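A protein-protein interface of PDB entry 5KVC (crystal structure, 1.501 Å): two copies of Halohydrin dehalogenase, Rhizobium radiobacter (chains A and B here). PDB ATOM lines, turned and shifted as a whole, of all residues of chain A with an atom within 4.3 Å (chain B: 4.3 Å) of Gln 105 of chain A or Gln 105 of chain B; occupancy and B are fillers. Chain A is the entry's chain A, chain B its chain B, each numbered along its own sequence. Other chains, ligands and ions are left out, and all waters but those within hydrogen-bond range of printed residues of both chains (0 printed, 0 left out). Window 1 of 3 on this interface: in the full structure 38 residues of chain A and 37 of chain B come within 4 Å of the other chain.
The side-chain amide nitrogen (NE2) of Gln 105 of chain B lies within hydrogen-bond range of the side-chain hydroxyl (OH) of Tyr 97 of chain A (3.1 Å).
NE2 of Gln 105 of chain A sits at hydrogen-bond distance from OH of Tyr 97 of chain B.
NE2 of Gln 105 of chain B sits at hydrogen-bond distance from OE1 of Gln 105 of chain A.
The backbone carbonyl oxygen (O) of Val 101 of chain A lies within hydrogen-bond range of the backbone NH (N) of Ile 106 of chain A (3.0 Å).
O of Val 101 of chain B sits at hydrogen-bond distance from N of Ile 106 of chain B.
CD1 of Ile 106 of chain B touches CD2 of Tyr 97 of chain A, at 3.5 Å.
CD2 of Tyr 97 of chain A touches CG of Phe 109 of chain B (3.3 Å).
Val 101 of chain A touches Val 101 of chain B.
Gln 105 of chain A touches Val 101 of chain B (NE2 to CG1, 3.9 Å).
CD1 of Ile 106 of chain A touches CD2 of Tyr 97 of chain B, at 3.5 Å.
Phe 109 of chain A touches Tyr 97 of chain B (CG to CD2, 3.3 Å).
Printed residues of chain B within 4 Å of Val 101 of chain A: Val 101.
Of the printed residues of chain B, Gln 105 of chain A touches Tyr 97 (3.1 Å), Val 101 (3.9 Å) and Gln 105 (2.9 Å).
Printed residues of chain B within 4 Å of Phe 109 of chain A: Tyr 97 (3.3 Å).
Of the printed residues of chain A, Tyr 97 of chain B touches Gln 105 (3.1 Å), Ile 106 (3.5 Å) and Phe 109 (3.3 Å).
Of the printed residues of chain A, Gln 105 of chain B touches Tyr 97 and Gln 105.
Of the printed residues of chain A, Ile 106 of chain B touches Tyr 97 (3.5 Å).
Of the printed residues of chain A, Phe 109 of chain B touches Tyr 97 (3.3 Å).
The nearest printed residue of chain B that does not touch Gln 105 of chain A is Ala 148 of chain B (4.6 Å).
The nearest printed residue of chain A that does not touch Gln 105 of chain B is Val 101 of chain A (4.1 Å).
The nearest printed residue of chain B that does not touch Phe 109 of chain A is Val 101 of chain B (8.0 Å).
Hydrophobic or aromatic side chains of chain B that line the printed part of chain A: Tyr 97, Val 101, Ile 106 and Phe 109.
Among the printed residues, 9 pairs touch across the chains.
Among the printed residues, no Asp or Glu carboxylate lies within 4 Å of a Lys or Arg side-chain nitrogen of the other chain.
Tyr 97 of chain A touches Ile 106 of chain B, and with the chains exchanged Ile 106 of chain A touches Tyr 97 of chain B.
Tyr 97 of chain A touches Phe 109 of chain B, and with the chains exchanged Phe 109 of chain A touches Tyr 97 of chain B.
Gln 105 of chain A touches Val 101 of chain B, but with the chains exchanged Val 101 of chain A does not touch Gln 105 of chain B (4.1 Å).
Gln 105 of chain A touches its own counterpart, Gln 105 of chain B.
Positions printed for both chains: 97, 101, 103, 104, 105, 106, 107, 108, 109, 148, 151, 152 and 155.
Of the 9 pairs that touch across the chains among the printed residues, 8 have their exchanged pair printed and touching as well.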
ATOM      1  N   TYR A  97      -8.144 -15.325 -31.070  1.00  0.00           N
ATOM      2  CA  TYR A  97      -9.461 -15.430 -30.434  1.00  0.00           C
ATOM      3  C   TYR A  97      -9.631 -16.772 -29.762  1.00  0.00           C
ATOM      4  O   TYR A  97     -10.157 -16.864 -28.639  1.00  0.00           O
ATOM      5  CB  TYR A  97     -10.554 -15.226 -31.475  1.00  0.00           C
ATOM      6  CG  TYR A  97     -11.962 -14.956 -30.914  1.00  0.00           C
ATOM      7  CD1 TYR A  97     -12.137 -14.345 -29.669  1.00  0.00           C
ATOM      8  CD2 TYR A  97     -13.084 -15.271 -31.676  1.00  0.00           C
ATOM      9  CE1 TYR A  97     -13.428 -14.063 -29.193  1.00  0.00           C
ATOM     10  CE2 TYR A  97     -14.369 -14.970 -31.226  1.00  0.00           C
ATOM     11  CZ  TYR A  97     -14.507 -14.380 -29.984  1.00  0.00           C
ATOM     12  OH  TYR A  97     -15.814 -14.064 -29.522  1.00  0.00           O
ATOM     13  N   ALA A 100      -8.141 -16.782 -26.328  1.00  0.00           N
ATOM     14  CA  ALA A 100      -8.939 -16.055 -25.340  1.00  0.00           C
ATOM     15  C   ALA A 100     -10.152 -16.872 -24.904  1.00  0.00           C
ATOM     16  O   ALA A 100     -10.437 -16.962 -23.707  1.00  0.00           O
ATOM     17  CB  ALA A 100      -9.403 -14.717 -25.915  1.00  0.00           C
ATOM     18  N   VAL A 101     -10.863 -17.468 -25.868  1.00  0.00           N
ATOM     19  CA  VAL A 101     -12.018 -18.307 -25.548  1.00  0.00           C
ATOM     20  C   VAL A 101     -11.573 -19.497 -24.705  1.00  0.00           C
ATOM     21  O   VAL A 101     -12.182 -19.820 -23.679  1.00  0.00           O
ATOM     22  CB  VAL A 101     -12.714 -18.753 -26.847  1.00  0.00           C
ATOM     23  CG1 VAL A 101     -13.827 -19.708 -26.573  1.00  0.00           C
ATOM     24  CG2 VAL A 101     -13.256 -17.545 -27.630  1.00  0.00           C
ATOM     25  N   ALA A 103      -9.062 -19.776 -22.591  1.00  0.00           N
ATOM     26  CA  ALA A 103      -8.676 -19.392 -21.243  1.00  0.00           C
ATOM     27  C   ALA A 103      -9.839 -18.834 -20.440  1.00  0.00           C
ATOM     28  O   ALA A 103      -9.844 -18.941 -19.202  1.00  0.00           O
ATOM     29  CB  ALA A 103      -7.554 -18.343 -21.297  1.00  0.00           C
ATOM     30  N   LEU A 104     -10.769 -18.153 -21.126  1.00  0.00           N
ATOM     31  CA  LEU A 104     -11.758 -17.366 -20.420  1.00  0.00           C
ATOM     32  C   LEU A 104     -13.165 -17.956 -20.461  1.00  0.00           C
ATOM     33  O   LEU A 104     -13.974 -17.569 -19.627  1.00  0.00           O
ATOM     34  CB  LEU A 104     -11.789 -15.929 -20.981  1.00  0.00           C
ATOM     35  CG  LEU A 104     -10.413 -15.239 -20.902  1.00  0.00           C
ATOM     36  CD1 LEU A 104     -10.557 -13.801 -21.497  1.00  0.00           C
ATOM     37  CD2 LEU A 104      -9.888 -15.226 -19.487  1.00  0.00           C
ATOM     38  N   GLN A 105     -13.463 -18.875 -21.384  1.00  0.00           N
ATOM     39  CA  GLN A 105     -14.743 -19.579 -21.426  1.00  0.00           C
ATOM     40  C   GLN A 105     -14.595 -21.070 -21.236  1.00  0.00           C
ATOM     41  O   GLN A 105     -15.310 -21.632 -20.409  1.00  0.00           O
ATOM     42  CB  GLN A 105     -15.451 -19.349 -22.760  1.00  0.00           C
ATOM     43  CG  GLN A 105     -16.031 -17.928 -22.949  1.00  0.00           C
ATOM     44  CD  GLN A 105     -16.549 -17.725 -24.354  1.00  0.00           C
ATOM     45  OE1 GLN A 105     -15.917 -17.067 -25.163  1.00  0.00           O
ATOM     46  NE2 GLN A 105     -17.679 -18.323 -24.670  1.00  0.00           N
ATOM     47  N   ILE A 106     -13.750 -21.730 -22.045  1.00  0.00           N
ATOM     48  CA  ILE A 106     -13.674 -23.185 -21.960  1.00  0.00           C
ATOM     49  C   ILE A 106     -13.181 -23.601 -20.581  1.00  0.00           C
ATOM     50  O   ILE A 106     -13.692 -24.558 -19.998  1.00  0.00           O
ATOM     51  CB  ILE A 106     -12.780 -23.751 -23.077  1.00  0.00           C
ATOM     52  CG1 ILE A 106     -13.170 -23.283 -24.478  1.00  0.00           C
ATOM     53  CG2 ILE A 106     -12.785 -25.298 -23.014  1.00  0.00           C
ATOM     54  CD1 ILE A 106     -14.627 -23.525 -24.900  1.00  0.00           C
ATOM     55  N   ARG A 107     -12.228 -22.860 -20.005  1.00  0.00           N
ATOM     56  CA  ARG A 107     -11.680 -23.239 -18.701  1.00  0.00           C
ATOM     57  C   ARG A 107     -12.725 -23.218 -17.583  1.00  0.00           C
ATOM     58  O   ARG A 107     -12.880 -24.244 -16.893  1.00  0.00           O
ATOM     59  CB  ARG A 107     -10.473 -22.345 -18.386  1.00  0.00           C
ATOM     60  CG  ARG A 107      -9.856 -22.609 -17.019  1.00  0.00           C
ATOM     61  CD  ARG A 107      -9.503 -24.125 -16.841  1.00  0.00           C
ATOM     62  NE  ARG A 107      -8.703 -24.619 -17.965  1.00  0.00           N
ATOM     63  CZ  ARG A 107      -7.436 -25.042 -17.875  1.00  0.00           C
ATOM     64  NH1 ARG A 107      -6.788 -25.453 -18.963  1.00  0.00           N
ATOM     65  NH2 ARG A 107      -6.823 -25.102 -16.708  1.00  0.00           N
ATOM     66  N   PRO A 108     -13.488 -22.138 -17.353  1.00  0.00           N
ATOM     67  CA  PRO A 108     -14.505 -22.239 -16.295  1.00  0.00           C
ATOM     68  C   PRO A 108     -15.560 -23.287 -16.618  1.00  0.00           C
ATOM     69  O   PRO A 108     -16.058 -23.968 -15.707  1.00  0.00           O
ATOM     70  CB  PRO A 108     -15.086 -20.810 -16.212  1.00  0.00           C
ATOM     71  CG  PRO A 108     -14.701 -20.149 -17.533  1.00  0.00           C
ATOM     72  CD  PRO A 108     -13.363 -20.760 -17.885  1.00  0.00           C
ATOM     73  N   PHE A 109     -15.921 -23.440 -17.890  1.00  0.00           N
ATOM     74  CA  PHE A 109     -16.873 -24.480 -18.255  1.00  0.00           C
ATOM     75  C   PHE A 109     -16.336 -25.840 -17.848  1.00  0.00           C
ATOM     76  O   PHE A 109     -17.082 -26.667 -17.294  1.00  0.00           O
ATOM     77  CB  PHE A 109     -17.140 -24.450 -19.755  1.00  0.00           C
ATOM     78  CG  PHE A 109     -18.110 -25.522 -20.239  1.00  0.00           C
ATOM     79  CD1 PHE A 109     -17.678 -26.837 -20.513  1.00  0.00           C
ATOM     80  CD2 PHE A 109     -19.449 -25.205 -20.435  1.00  0.00           C
ATOM     81  CE1 PHE A 109     -18.597 -27.786 -20.983  1.00  0.00           C
ATOM     82  CE2 PHE A 109     -20.385 -26.136 -20.889  1.00  0.00           C
ATOM     83  CZ  PHE A 109     -19.949 -27.440 -21.149  1.00  0.00           C
ATOM     84  N   ALA A 148     -14.988 -12.834 -25.054  1.00  0.00           N
ATOM     85  CA  ALA A 148     -14.873 -14.082 -24.302  1.00  0.00           C
ATOM     86  C   ALA A 148     -15.336 -13.909 -22.866  1.00  0.00           C
ATOM     87  O   ALA A 148     -16.048 -14.768 -22.333  1.00  0.00           O
ATOM     88  CB  ALA A 148     -13.428 -14.613 -24.366  1.00  0.00           C
ATOM     89  N   GLY A 151     -19.022 -14.077 -22.747  1.00  0.00           N
ATOM     90  CA  GLY A 151     -19.456 -15.472 -22.799  1.00  0.00           C
ATOM     91  C   GLY A 151     -19.430 -16.122 -21.435  1.00  0.00           C
ATOM     92  O   GLY A 151     -20.325 -16.907 -21.084  1.00  0.00           O
ATOM     93  N   ALA A 152     -18.372 -15.854 -20.656  1.00  0.00           N
ATOM     94  CA  ALA A 152     -18.271 -16.436 -19.320  1.00  0.00           C
ATOM     95  C   ALA A 152     -19.337 -15.885 -18.384  1.00  0.00           C
ATOM     96  O   ALA A 152     -19.894 -16.626 -17.567  1.00  0.00           O
ATOM     97  CB  ALA A 152     -16.884 -16.160 -18.742  1.00  0.00           C
ATOM     98  N   LEU A 155     -22.443 -17.635 -19.306  1.00  0.00           N
ATOM     99  CA  LEU A 155     -22.328 -19.018 -18.814  1.00  0.00           C
ATOM    100  C   LEU A 155     -22.729 -19.112 -17.341  1.00  0.00           C
ATOM    101  O   LEU A 155     -23.543 -19.970 -16.968  1.00  0.00           O
ATOM    102  CB  LEU A 155     -20.875 -19.501 -19.030  1.00  0.00           C
ATOM    103  CG  LEU A 155     -20.637 -20.958 -18.571  1.00  0.00           C
ATOM    104  CD1 LEU A 155     -21.580 -21.941 -19.235  1.00  0.00           C
ATOM    105  CD2 LEU A 155     -19.116 -21.354 -18.838  1.00  0.00           C
ATOM    106  N   TYR B  97     -18.725 -27.845 -25.807  1.00  0.00           N
ATOM    107  CA  TYR B  97     -18.646 -26.387 -25.729  1.00  0.00           C
ATOM    108  C   TYR B  97     -17.729 -25.828 -26.799  1.00  0.00           C
ATOM    109  O   TYR B  97     -18.063 -24.819 -27.425  1.00  0.00           O
ATOM    110  CB  TYR B  97     -18.182 -25.957 -24.352  1.00  0.00           C
ATOM    111  CG  TYR B  97     -18.399 -24.470 -24.032  1.00  0.00           C
ATOM    112  CD1 TYR B  97     -19.420 -23.731 -24.635  1.00  0.00           C
ATOM    113  CD2 TYR B  97     -17.626 -23.852 -23.069  1.00  0.00           C
ATOM    114  CE1 TYR B  97     -19.629 -22.377 -24.267  1.00  0.00           C
ATOM    115  CE2 TYR B  97     -17.803 -22.537 -22.715  1.00  0.00           C
ATOM    116  CZ  TYR B  97     -18.836 -21.831 -23.304  1.00  0.00           C
ATOM    117  OH  TYR B  97     -18.996 -20.514 -22.876  1.00  0.00           O
ATOM    118  N   VAL B 101     -18.649 -22.862 -29.506  1.00  0.00           N
ATOM    119  CA  VAL B 101     -17.954 -21.584 -29.680  1.00  0.00           C
ATOM    120  C   VAL B 101     -17.309 -21.517 -31.056  1.00  0.00           C
ATOM    121  O   VAL B 101     -17.255 -20.445 -31.673  1.00  0.00           O
ATOM    122  CB  VAL B 101     -16.930 -21.300 -28.558  1.00  0.00           C
ATOM    123  CG1 VAL B 101     -17.565 -21.369 -27.159  1.00  0.00           C
ATOM    124  CG2 VAL B 101     -15.697 -22.193 -28.636  1.00  0.00           C
ATOM    125  N   ALA B 103     -18.548 -22.712 -33.864  1.00  0.00           N
ATOM    126  CA  ALA B 103     -19.584 -22.381 -34.830  1.00  0.00           C
ATOM    127  C   ALA B 103     -20.180 -20.991 -34.621  1.00  0.00           C
ATOM    128  O   ALA B 103     -20.644 -20.381 -35.586  1.00  0.00           O
ATOM    129  CB  ALA B 103     -20.736 -23.394 -34.739  1.00  0.00           C
ATOM    130  N   LEU B 104     -20.269 -20.533 -33.363  1.00  0.00           N
ATOM    131  CA  LEU B 104     -21.075 -19.348 -33.073  1.00  0.00           C
ATOM    132  C   LEU B 104     -20.273 -18.115 -32.695  1.00  0.00           C
ATOM    133  O   LEU B 104     -20.832 -16.998 -32.735  1.00  0.00           O
ATOM    134  CB  LEU B 104     -22.075 -19.681 -31.959  1.00  0.00           C
ATOM    135  CG  LEU B 104     -22.993 -20.870 -32.259  1.00  0.00           C
ATOM    136  CD1 LEU B 104     -23.852 -21.130 -30.997  1.00  0.00           C
ATOM    137  CD2 LEU B 104     -23.807 -20.586 -33.531  1.00  0.00           C
ATOM    138  N   GLN B 105     -18.987 -18.278 -32.358  1.00  0.00           N
ATOM    139  CA  GLN B 105     -18.100 -17.153 -32.056  1.00  0.00           C
ATOM    140  C   GLN B 105     -16.899 -17.100 -32.979  1.00  0.00           C
ATOM    141  O   GLN B 105     -16.605 -16.039 -33.543  1.00  0.00           O
ATOM    142  CB  GLN B 105     -17.562 -17.231 -30.620  1.00  0.00           C
ATOM    143  CG  GLN B 105     -18.583 -16.875 -29.561  1.00  0.00           C
ATOM    144  CD  GLN B 105     -18.023 -17.108 -28.172  1.00  0.00           C
ATOM    145  OE1 GLN B 105     -18.384 -18.077 -27.512  1.00  0.00           O
ATOM    146  NE2 GLN B 105     -17.114 -16.228 -27.709  1.00  0.00           N
ATOM    147  N   ILE B 106     -16.170 -18.216 -33.112  1.00  0.00           N
ATOM    148  CA  ILE B 106     -14.952 -18.176 -33.921  1.00  0.00           C
ATOM    149  C   ILE B 106     -15.298 -17.879 -35.365  1.00  0.00           C
ATOM    150  O   ILE B 106     -14.589 -17.108 -36.037  1.00  0.00           O
ATOM    151  CB  ILE B 106     -14.153 -19.492 -33.783  1.00  0.00           C
ATOM    152  CG1 ILE B 106     -13.841 -19.853 -32.333  1.00  0.00           C
ATOM    153  CG2 ILE B 106     -12.826 -19.393 -34.548  1.00  0.00           C
ATOM    154  CD1 ILE B 106     -13.073 -18.803 -31.516  1.00  0.00           C
ATOM    155  N   ARG B 107     -16.387 -18.470 -35.876  1.00  0.00           N
ATOM    156  CA  ARG B 107     -16.727 -18.257 -37.284  1.00  0.00           C
ATOM    157  C   ARG B 107     -17.066 -16.805 -37.614  1.00  0.00           C
ATOM    158  O   ARG B 107     -16.452 -16.250 -38.544  1.00  0.00           O
ATOM    159  CB  ARG B 107     -17.837 -19.230 -37.697  1.00  0.00           C
ATOM    160  CG  ARG B 107     -18.307 -19.088 -39.135  1.00  0.00           C
ATOM    161  CD  ARG B 107     -17.150 -19.052 -40.165  1.00  0.00           C
ATOM    162  NE  ARG B 107     -16.340 -20.266 -40.142  1.00  0.00           N
ATOM    163  CZ  ARG B 107     -16.565 -21.329 -40.921  1.00  0.00           C
ATOM    164  NH1 ARG B 107     -15.782 -22.391 -40.832  1.00  0.00           N
ATOM    165  NH2 ARG B 107     -17.574 -21.324 -41.778  1.00  0.00           N
ATOM    166  N   PRO B 108     -17.954 -16.108 -36.892  1.00  0.00           N
ATOM    167  CA  PRO B 108     -18.169 -14.697 -37.247  1.00  0.00           C
ATOM    168  C   PRO B 108     -16.886 -13.890 -37.072  1.00  0.00           C
ATOM    169  O   PRO B 108     -16.613 -13.006 -37.900  1.00  0.00           O
ATOM    170  CB  PRO B 108     -19.318 -14.256 -36.314  1.00  0.00           C
ATOM    171  CG  PRO B 108     -19.396 -15.300 -35.223  1.00  0.00           C
ATOM    172  CD  PRO B 108     -18.920 -16.604 -35.878  1.00  0.00           C
ATOM    173  N   PHE B 109     -16.107 -14.181 -36.029  1.00  0.00           N
ATOM    174  CA  PHE B 109     -14.816 -13.507 -35.849  1.00  0.00           C
ATOM    175  C   PHE B 109     -13.933 -13.687 -37.074  1.00  0.00           C
ATOM    176  O   PHE B 109     -13.354 -12.720 -37.572  1.00  0.00           O
ATOM    177  CB  PHE B 109     -14.099 -14.039 -34.624  1.00  0.00           C
ATOM    178  CG  PHE B 109     -12.789 -13.355 -34.342  1.00  0.00           C
ATOM    179  CD1 PHE B 109     -11.607 -13.744 -34.995  1.00  0.00           C
ATOM    180  CD2 PHE B 109     -12.724 -12.319 -33.408  1.00  0.00           C
ATOM    181  CE1 PHE B 109     -10.385 -13.080 -34.727  1.00  0.00           C
ATOM    182  CE2 PHE B 109     -11.506 -11.660 -33.139  1.00  0.00           C
ATOM    183  CZ  PHE B 109     -10.338 -12.057 -33.786  1.00  0.00           C
ATOM    184  N   ALA B 148     -22.258 -19.079 -25.891  1.00  0.00           N
ATOM    185  CA  ALA B 148     -21.548 -18.744 -27.125  1.00  0.00           C
ATOM    186  C   ALA B 148     -22.262 -17.634 -27.899  1.00  0.00           C
ATOM    187  O   ALA B 148     -21.614 -16.719 -28.419  1.00  0.00           O
ATOM    188  CB  ALA B 148     -21.362 -20.005 -27.986  1.00  0.00           C
ATOM    189  N   GLY B 151     -21.388 -14.354 -26.391  1.00  0.00           N
ATOM    190  CA  GLY B 151     -20.072 -13.939 -26.885  1.00  0.00           C
ATOM    191  C   GLY B 151     -20.145 -13.248 -28.225  1.00  0.00           C
ATOM    192  O   GLY B 151     -19.422 -12.264 -28.464  1.00  0.00           O
ATOM    193  N   ALA B 152     -20.942 -13.793 -29.149  1.00  0.00           N
ATOM    194  CA  ALA B 152     -21.083 -13.193 -30.467  1.00  0.00           C
ATOM    195  C   ALA B 152     -21.742 -11.816 -30.384  1.00  0.00           C
ATOM    196  O   ALA B 152     -21.359 -10.885 -31.102  1.00  0.00           O
ATOM    197  CB  ALA B 152     -21.887 -14.141 -31.372  1.00  0.00           C
ATOM    198  N   LEU B 155     -19.195  -9.535 -29.172  1.00  0.00           N
ATOM    199  CA  LEU B 155     -18.230  -9.277 -30.243  1.00  0.00           C
ATOM    200  C   LEU B 155     -18.728  -8.178 -31.186  1.00  0.00           C
ATOM    201  O   LEU B 155     -17.975  -7.261 -31.532  1.00  0.00           O
ATOM    202  CB  LEU B 155     -17.958 -10.602 -30.990  1.00  0.00           C
ATOM    203  CG  LEU B 155     -17.018 -10.492 -32.207  1.00  0.00           C
ATOM    204  CD1 LEU B 155     -15.624  -9.956 -31.809  1.00  0.00           C
ATOM    205  CD2 LEU B 155     -16.918 -11.868 -32.907  1.00  0.00           C
